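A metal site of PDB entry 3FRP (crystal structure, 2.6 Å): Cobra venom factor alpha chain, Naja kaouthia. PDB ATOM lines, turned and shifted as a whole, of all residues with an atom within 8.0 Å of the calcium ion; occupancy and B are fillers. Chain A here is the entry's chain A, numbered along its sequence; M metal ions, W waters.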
ATOM      1  N   LYS A 327       2.954  16.711  -5.733  1.00  0.00           N
ATOM      2  CA  LYS A 327       2.363  18.044  -5.804  1.00  0.00           C
ATOM      3  C   LYS A 327       1.648  18.328  -7.133  1.00  0.00           C
ATOM      4  O   LYS A 327       1.310  19.477  -7.392  1.00  0.00           O
ATOM      5  CB  LYS A 327       3.440  19.104  -5.532  1.00  0.00           C
ATOM      6  CG  LYS A 327       4.106  19.028  -4.152  1.00  0.00           C
ATOM      7  CD  LYS A 327       5.434  19.831  -4.115  1.00  0.00           C
ATOM      8  CE  LYS A 327       6.154  19.754  -2.755  1.00  0.00           C
ATOM      9  NZ  LYS A 327       5.399  20.439  -1.659  1.00  0.00           N
ATOM     10  N   ILE A 432       5.027  31.025  -3.013  1.00  0.00           N
ATOM     11  CA  ILE A 432       4.051  31.985  -2.487  1.00  0.00           C
ATOM     12  C   ILE A 432       4.325  32.324  -1.009  1.00  0.00           C
ATOM     13  O   ILE A 432       4.503  31.441  -0.171  1.00  0.00           O
ATOM     14  CB  ILE A 432       2.597  31.456  -2.697  1.00  0.00           C
ATOM     15  CG1 ILE A 432       2.406  30.900  -4.118  1.00  0.00           C
ATOM     16  CG2 ILE A 432       1.550  32.531  -2.397  1.00  0.00           C
ATOM     17  CD1 ILE A 432       1.989  31.911  -5.154  1.00  0.00           C
ATOM     18  N   LEU A 492      -3.004  32.038   5.926  1.00  0.00           N
ATOM     19  CA  LEU A 492      -2.884  30.940   4.975  1.00  0.00           C
ATOM     20  C   LEU A 492      -1.647  30.062   5.161  1.00  0.00           C
ATOM     21  O   LEU A 492      -1.374  29.193   4.334  1.00  0.00           O
ATOM     22  CB  LEU A 492      -2.927  31.489   3.544  1.00  0.00           C
ATOM     23  CG  LEU A 492      -4.216  32.256   3.233  1.00  0.00           C
ATOM     24  CD1 LEU A 492      -4.275  32.616   1.758  1.00  0.00           C
ATOM     25  CD2 LEU A 492      -5.481  31.475   3.657  1.00  0.00           C
ATOM     26  N   ILE A 493      -0.896  30.276   6.223  1.00  0.00           N
ATOM     27  CA  ILE A 493       0.275  29.460   6.482  1.00  0.00           C
ATOM     28  C   ILE A 493      -0.275  28.166   7.068  1.00  0.00           C
ATOM     29  O   ILE A 493      -1.252  28.203   7.811  1.00  0.00           O
ATOM     30  CB  ILE A 493       1.265  30.183   7.444  1.00  0.00           C
ATOM     31  CG1 ILE A 493       1.868  31.416   6.757  1.00  0.00           C
ATOM     32  CG2 ILE A 493       2.407  29.277   7.892  1.00  0.00           C
ATOM     33  CD1 ILE A 493       2.591  32.352   7.718  1.00  0.00           C
ATOM     34  N   PRO A 494       0.311  27.002   6.726  1.00  0.00           N
ATOM     35  CA  PRO A 494       1.480  26.718   5.891  1.00  0.00           C
ATOM     36  C   PRO A 494       1.162  26.493   4.409  1.00  0.00           C
ATOM     37  O   PRO A 494       2.090  26.391   3.595  1.00  0.00           O
ATOM     38  CB  PRO A 494       2.028  25.428   6.510  1.00  0.00           C
ATOM     39  CG  PRO A 494       0.882  24.798   7.225  1.00  0.00           C
ATOM     40  CD  PRO A 494      -0.244  25.777   7.330  1.00  0.00           C
ATOM     41  N   SER A 495      -0.115  26.407   4.073  1.00  0.00           N
ATOM     42  CA  SER A 495      -0.624  26.112   2.723  1.00  0.00           C
ATOM     43  C   SER A 495      -2.107  26.215   2.791  1.00  0.00           C
ATOM     44  O   SER A 495      -2.699  25.974   3.826  1.00  0.00           O
ATOM     45  CB  SER A 495      -0.298  24.678   2.293  1.00  0.00           C
ATOM     46  OG  SER A 495      -1.013  23.732   3.081  1.00  0.00           O
ATOM     47  N   PHE A 496      -2.713  26.540   1.662  1.00  0.00           N
ATOM     48  CA  PHE A 496      -4.165  26.546   1.588  1.00  0.00           C
ATOM     49  C   PHE A 496      -4.641  25.794   0.329  1.00  0.00           C
ATOM     50  O   PHE A 496      -3.856  25.531  -0.594  1.00  0.00           O
ATOM     51  CB  PHE A 496      -4.658  27.994   1.580  1.00  0.00           C
ATOM     52  CG  PHE A 496      -4.244  28.773   0.372  1.00  0.00           C
ATOM     53  CD1 PHE A 496      -2.994  29.408   0.331  1.00  0.00           C
ATOM     54  CD2 PHE A 496      -5.089  28.878  -0.733  1.00  0.00           C
ATOM     55  CE1 PHE A 496      -2.583  30.125  -0.782  1.00  0.00           C
ATOM     56  CE2 PHE A 496      -4.694  29.607  -1.855  1.00  0.00           C
ATOM     57  CZ  PHE A 496      -3.435  30.223  -1.884  1.00  0.00           C
ATOM     58  N   TRP A 515      -3.807  22.953  -4.934  1.00  0.00           N
ATOM     59  CA  TRP A 515      -3.094  23.070  -3.650  1.00  0.00           C
ATOM     60  C   TRP A 515      -1.968  24.081  -3.730  1.00  0.00           C
ATOM     61  O   TRP A 515      -1.030  23.917  -4.534  1.00  0.00           O
ATOM     62  CB  TRP A 515      -2.508  21.732  -3.256  1.00  0.00           C
ATOM     63  CG  TRP A 515      -1.741  21.733  -1.949  1.00  0.00           C
ATOM     64  CD1 TRP A 515      -2.278  21.649  -0.696  1.00  0.00           C
ATOM     65  CD2 TRP A 515      -0.319  21.795  -1.769  1.00  0.00           C
ATOM     66  NE1 TRP A 515      -1.284  21.670   0.244  1.00  0.00           N
ATOM     67  CE2 TRP A 515      -0.076  21.757  -0.379  1.00  0.00           C
ATOM     68  CE3 TRP A 515       0.768  21.903  -2.653  1.00  0.00           C
ATOM     69  CZ2 TRP A 515       1.224  21.809   0.157  1.00  0.00           C
ATOM     70  CZ3 TRP A 515       2.069  21.970  -2.110  1.00  0.00           C
ATOM     71  CH2 TRP A 515       2.276  21.923  -0.722  1.00  0.00           C
ATOM     72  N   VAL A 516      -2.004  25.094  -2.871  1.00  0.00           N
ATOM     73  CA  VAL A 516      -0.984  26.138  -2.865  1.00  0.00           C
ATOM     74  C   VAL A 516      -0.157  26.173  -1.586  1.00  0.00           C
ATOM     75  O   VAL A 516      -0.683  26.404  -0.498  1.00  0.00           O
ATOM     76  CB  VAL A 516      -1.583  27.549  -3.095  1.00  0.00           C
ATOM     77  CG1 VAL A 516      -0.469  28.548  -3.398  1.00  0.00           C
ATOM     78  CG2 VAL A 516      -2.571  27.535  -4.233  1.00  0.00           C
ATOM     79  N   ASP A 517       1.140  25.934  -1.729  1.00  0.00           N
ATOM     80  CA  ASP A 517       2.078  26.012  -0.624  1.00  0.00           C
ATOM     81  C   ASP A 517       2.321  27.489  -0.267  1.00  0.00           C
ATOM     82  O   ASP A 517       2.315  28.350  -1.144  1.00  0.00           O
ATOM     83  CB  ASP A 517       3.392  25.302  -0.991  1.00  0.00           C
ATOM     84  CG  ASP A 517       4.190  24.844   0.241  1.00  0.00           C
ATOM     85  OD1 ASP A 517       3.888  25.292   1.371  1.00  0.00           O
ATOM     86  OD2 ASP A 517       5.113  24.030   0.091  1.00  0.00           O
ATOM     87  N   VAL A 518       2.530  27.775   1.016  1.00  0.00           N
ATOM     88  CA  VAL A 518       2.852  29.118   1.487  1.00  0.00           C
ATOM     89  C   VAL A 518       4.113  28.984   2.314  1.00  0.00           C
ATOM     90  O   VAL A 518       4.307  27.931   2.964  1.00  0.00           O
ATOM     91  CB  VAL A 518       1.718  29.726   2.357  1.00  0.00           C
ATOM     92  CG1 VAL A 518       2.129  31.061   2.886  1.00  0.00           C
ATOM     93  CG2 VAL A 518       0.426  29.856   1.558  1.00  0.00           C
ATOM     94  N   LYS A 519       4.965  30.012   2.302  1.00  0.00           N
ATOM     95  CA  LYS A 519       6.259  29.942   2.997  1.00  0.00           C
ATOM     96  C   LYS A 519       6.042  29.743   4.503  1.00  0.00           C
ATOM     97  O   LYS A 519       5.262  30.459   5.111  1.00  0.00           O
ATOM     98  CB  LYS A 519       7.040  31.215   2.724  1.00  0.00           C
ATOM     99  CG  LYS A 519       8.375  31.273   3.407  1.00  0.00           C
ATOM    100  CD  LYS A 519       8.972  32.672   3.269  1.00  0.00           C
ATOM    101  CE  LYS A 519      10.301  32.753   4.001  1.00  0.00           C
ATOM    102  NZ  LYS A 519      11.080  33.894   3.443  1.00  0.00           N
ATOM    103  N   ASP A 520       6.723  28.762   5.101  1.00  0.00           N
ATOM    104  CA  ASP A 520       6.481  28.450   6.509  1.00  0.00           C
ATOM    105  C   ASP A 520       7.304  29.317   7.464  1.00  0.00           C
ATOM    106  O   ASP A 520       8.381  28.892   7.915  1.00  0.00           O
ATOM    107  CB  ASP A 520       6.768  26.975   6.839  1.00  0.00           C
ATOM    108  CG  ASP A 520       6.074  26.025   5.917  1.00  0.00           C
ATOM    109  OD1 ASP A 520       4.919  26.312   5.549  1.00  0.00           O
ATOM    110  OD2 ASP A 520       6.678  24.995   5.556  1.00  0.00           O
ATOM    111  N   THR A 521       6.803  30.497   7.798  1.00  0.00           N
ATOM    112  CA  THR A 521       7.391  31.265   8.888  1.00  0.00           C
ATOM    113  C   THR A 521       6.485  31.243  10.126  1.00  0.00           C
ATOM    114  O   THR A 521       5.465  30.545  10.168  1.00  0.00           O
ATOM    115  CB  THR A 521       7.657  32.752   8.515  1.00  0.00           C
ATOM    116  OG1 THR A 521       6.415  33.409   8.258  1.00  0.00           O
ATOM    117  CG2 THR A 521       8.532  32.855   7.257  1.00  0.00           C
ATOM    118  N   TRP A 577       4.772  23.349  11.819  1.00  0.00           N
ATOM    119  CA  TRP A 577       4.134  23.382  10.514  1.00  0.00           C
ATOM    120  C   TRP A 577       4.060  21.995   9.870  1.00  0.00           C
ATOM    121  O   TRP A 577       3.111  21.703   9.129  1.00  0.00           O
ATOM    122  CB  TRP A 577       4.796  24.417   9.594  1.00  0.00           C
ATOM    123  CG  TRP A 577       4.591  25.832  10.056  1.00  0.00           C
ATOM    124  CD1 TRP A 577       5.560  26.766  10.289  1.00  0.00           C
ATOM    125  CD2 TRP A 577       3.347  26.487  10.338  1.00  0.00           C
ATOM    126  NE1 TRP A 577       5.000  27.957  10.694  1.00  0.00           N
ATOM    127  CE2 TRP A 577       3.635  27.807  10.737  1.00  0.00           C
ATOM    128  CE3 TRP A 577       2.009  26.077  10.291  1.00  0.00           C
ATOM    129  CZ2 TRP A 577       2.657  28.723  11.096  1.00  0.00           C
ATOM    130  CZ3 TRP A 577       1.027  26.989  10.630  1.00  0.00           C
ATOM    131  CH2 TRP A 577       1.357  28.296  11.024  1.00  0.00           C
ATOM    132  N   GLU A 581       0.415  20.244   8.767  1.00  0.00           N
ATOM    133  CA  GLU A 581       0.202  19.782   7.384  1.00  0.00           C
ATOM    134  C   GLU A 581      -0.177  18.307   7.341  1.00  0.00           C
ATOM    135  O   GLU A 581      -1.145  17.937   6.691  1.00  0.00           O
ATOM    136  CB  GLU A 581       1.456  19.961   6.507  1.00  0.00           C
ATOM    137  CG  GLU A 581       1.720  21.375   6.045  1.00  0.00           C
ATOM    138  CD  GLU A 581       0.990  21.729   4.788  1.00  0.00           C
ATOM    139  OE1 GLU A 581      -0.245  21.831   4.801  1.00  0.00           O
ATOM    140  OE2 GLU A 581       1.641  21.961   3.765  1.00  0.00           O
HETATM  141 CA    CA M   1       4.323  25.552   3.486  1.00  0.00          CA
HETATM  142  O   HOH W   1       3.967  23.163   4.337  1.00  0.00           O
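Along chain A the residues within 4 Å of the calcium ion span positions 494 to 520.
The nearest printed residue that does not touch the calcium ion is Glu 581 (4.5 Å).
The side-chain carboxylate (OD1) of Asp 517 binds the calcium ion (2.2 Å).
The side-chain carboxylate (OD1) of Asp 520 binds the calcium ion, at 2.3 Å.
The calcium ion is bound by O of Pro 494 (2.4 Å).
O of Val 518 binds the calcium ion, 2.4 Å away.
Water W1 binds the calcium ion (2.6 Å).
The calcium ion has five donor atoms within binding distance.
Water W1 lies within hydrogen-bond range of OE2 of Glu 581 (2.7 Å) and OD2 of Asp 520 (3.5 Å).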
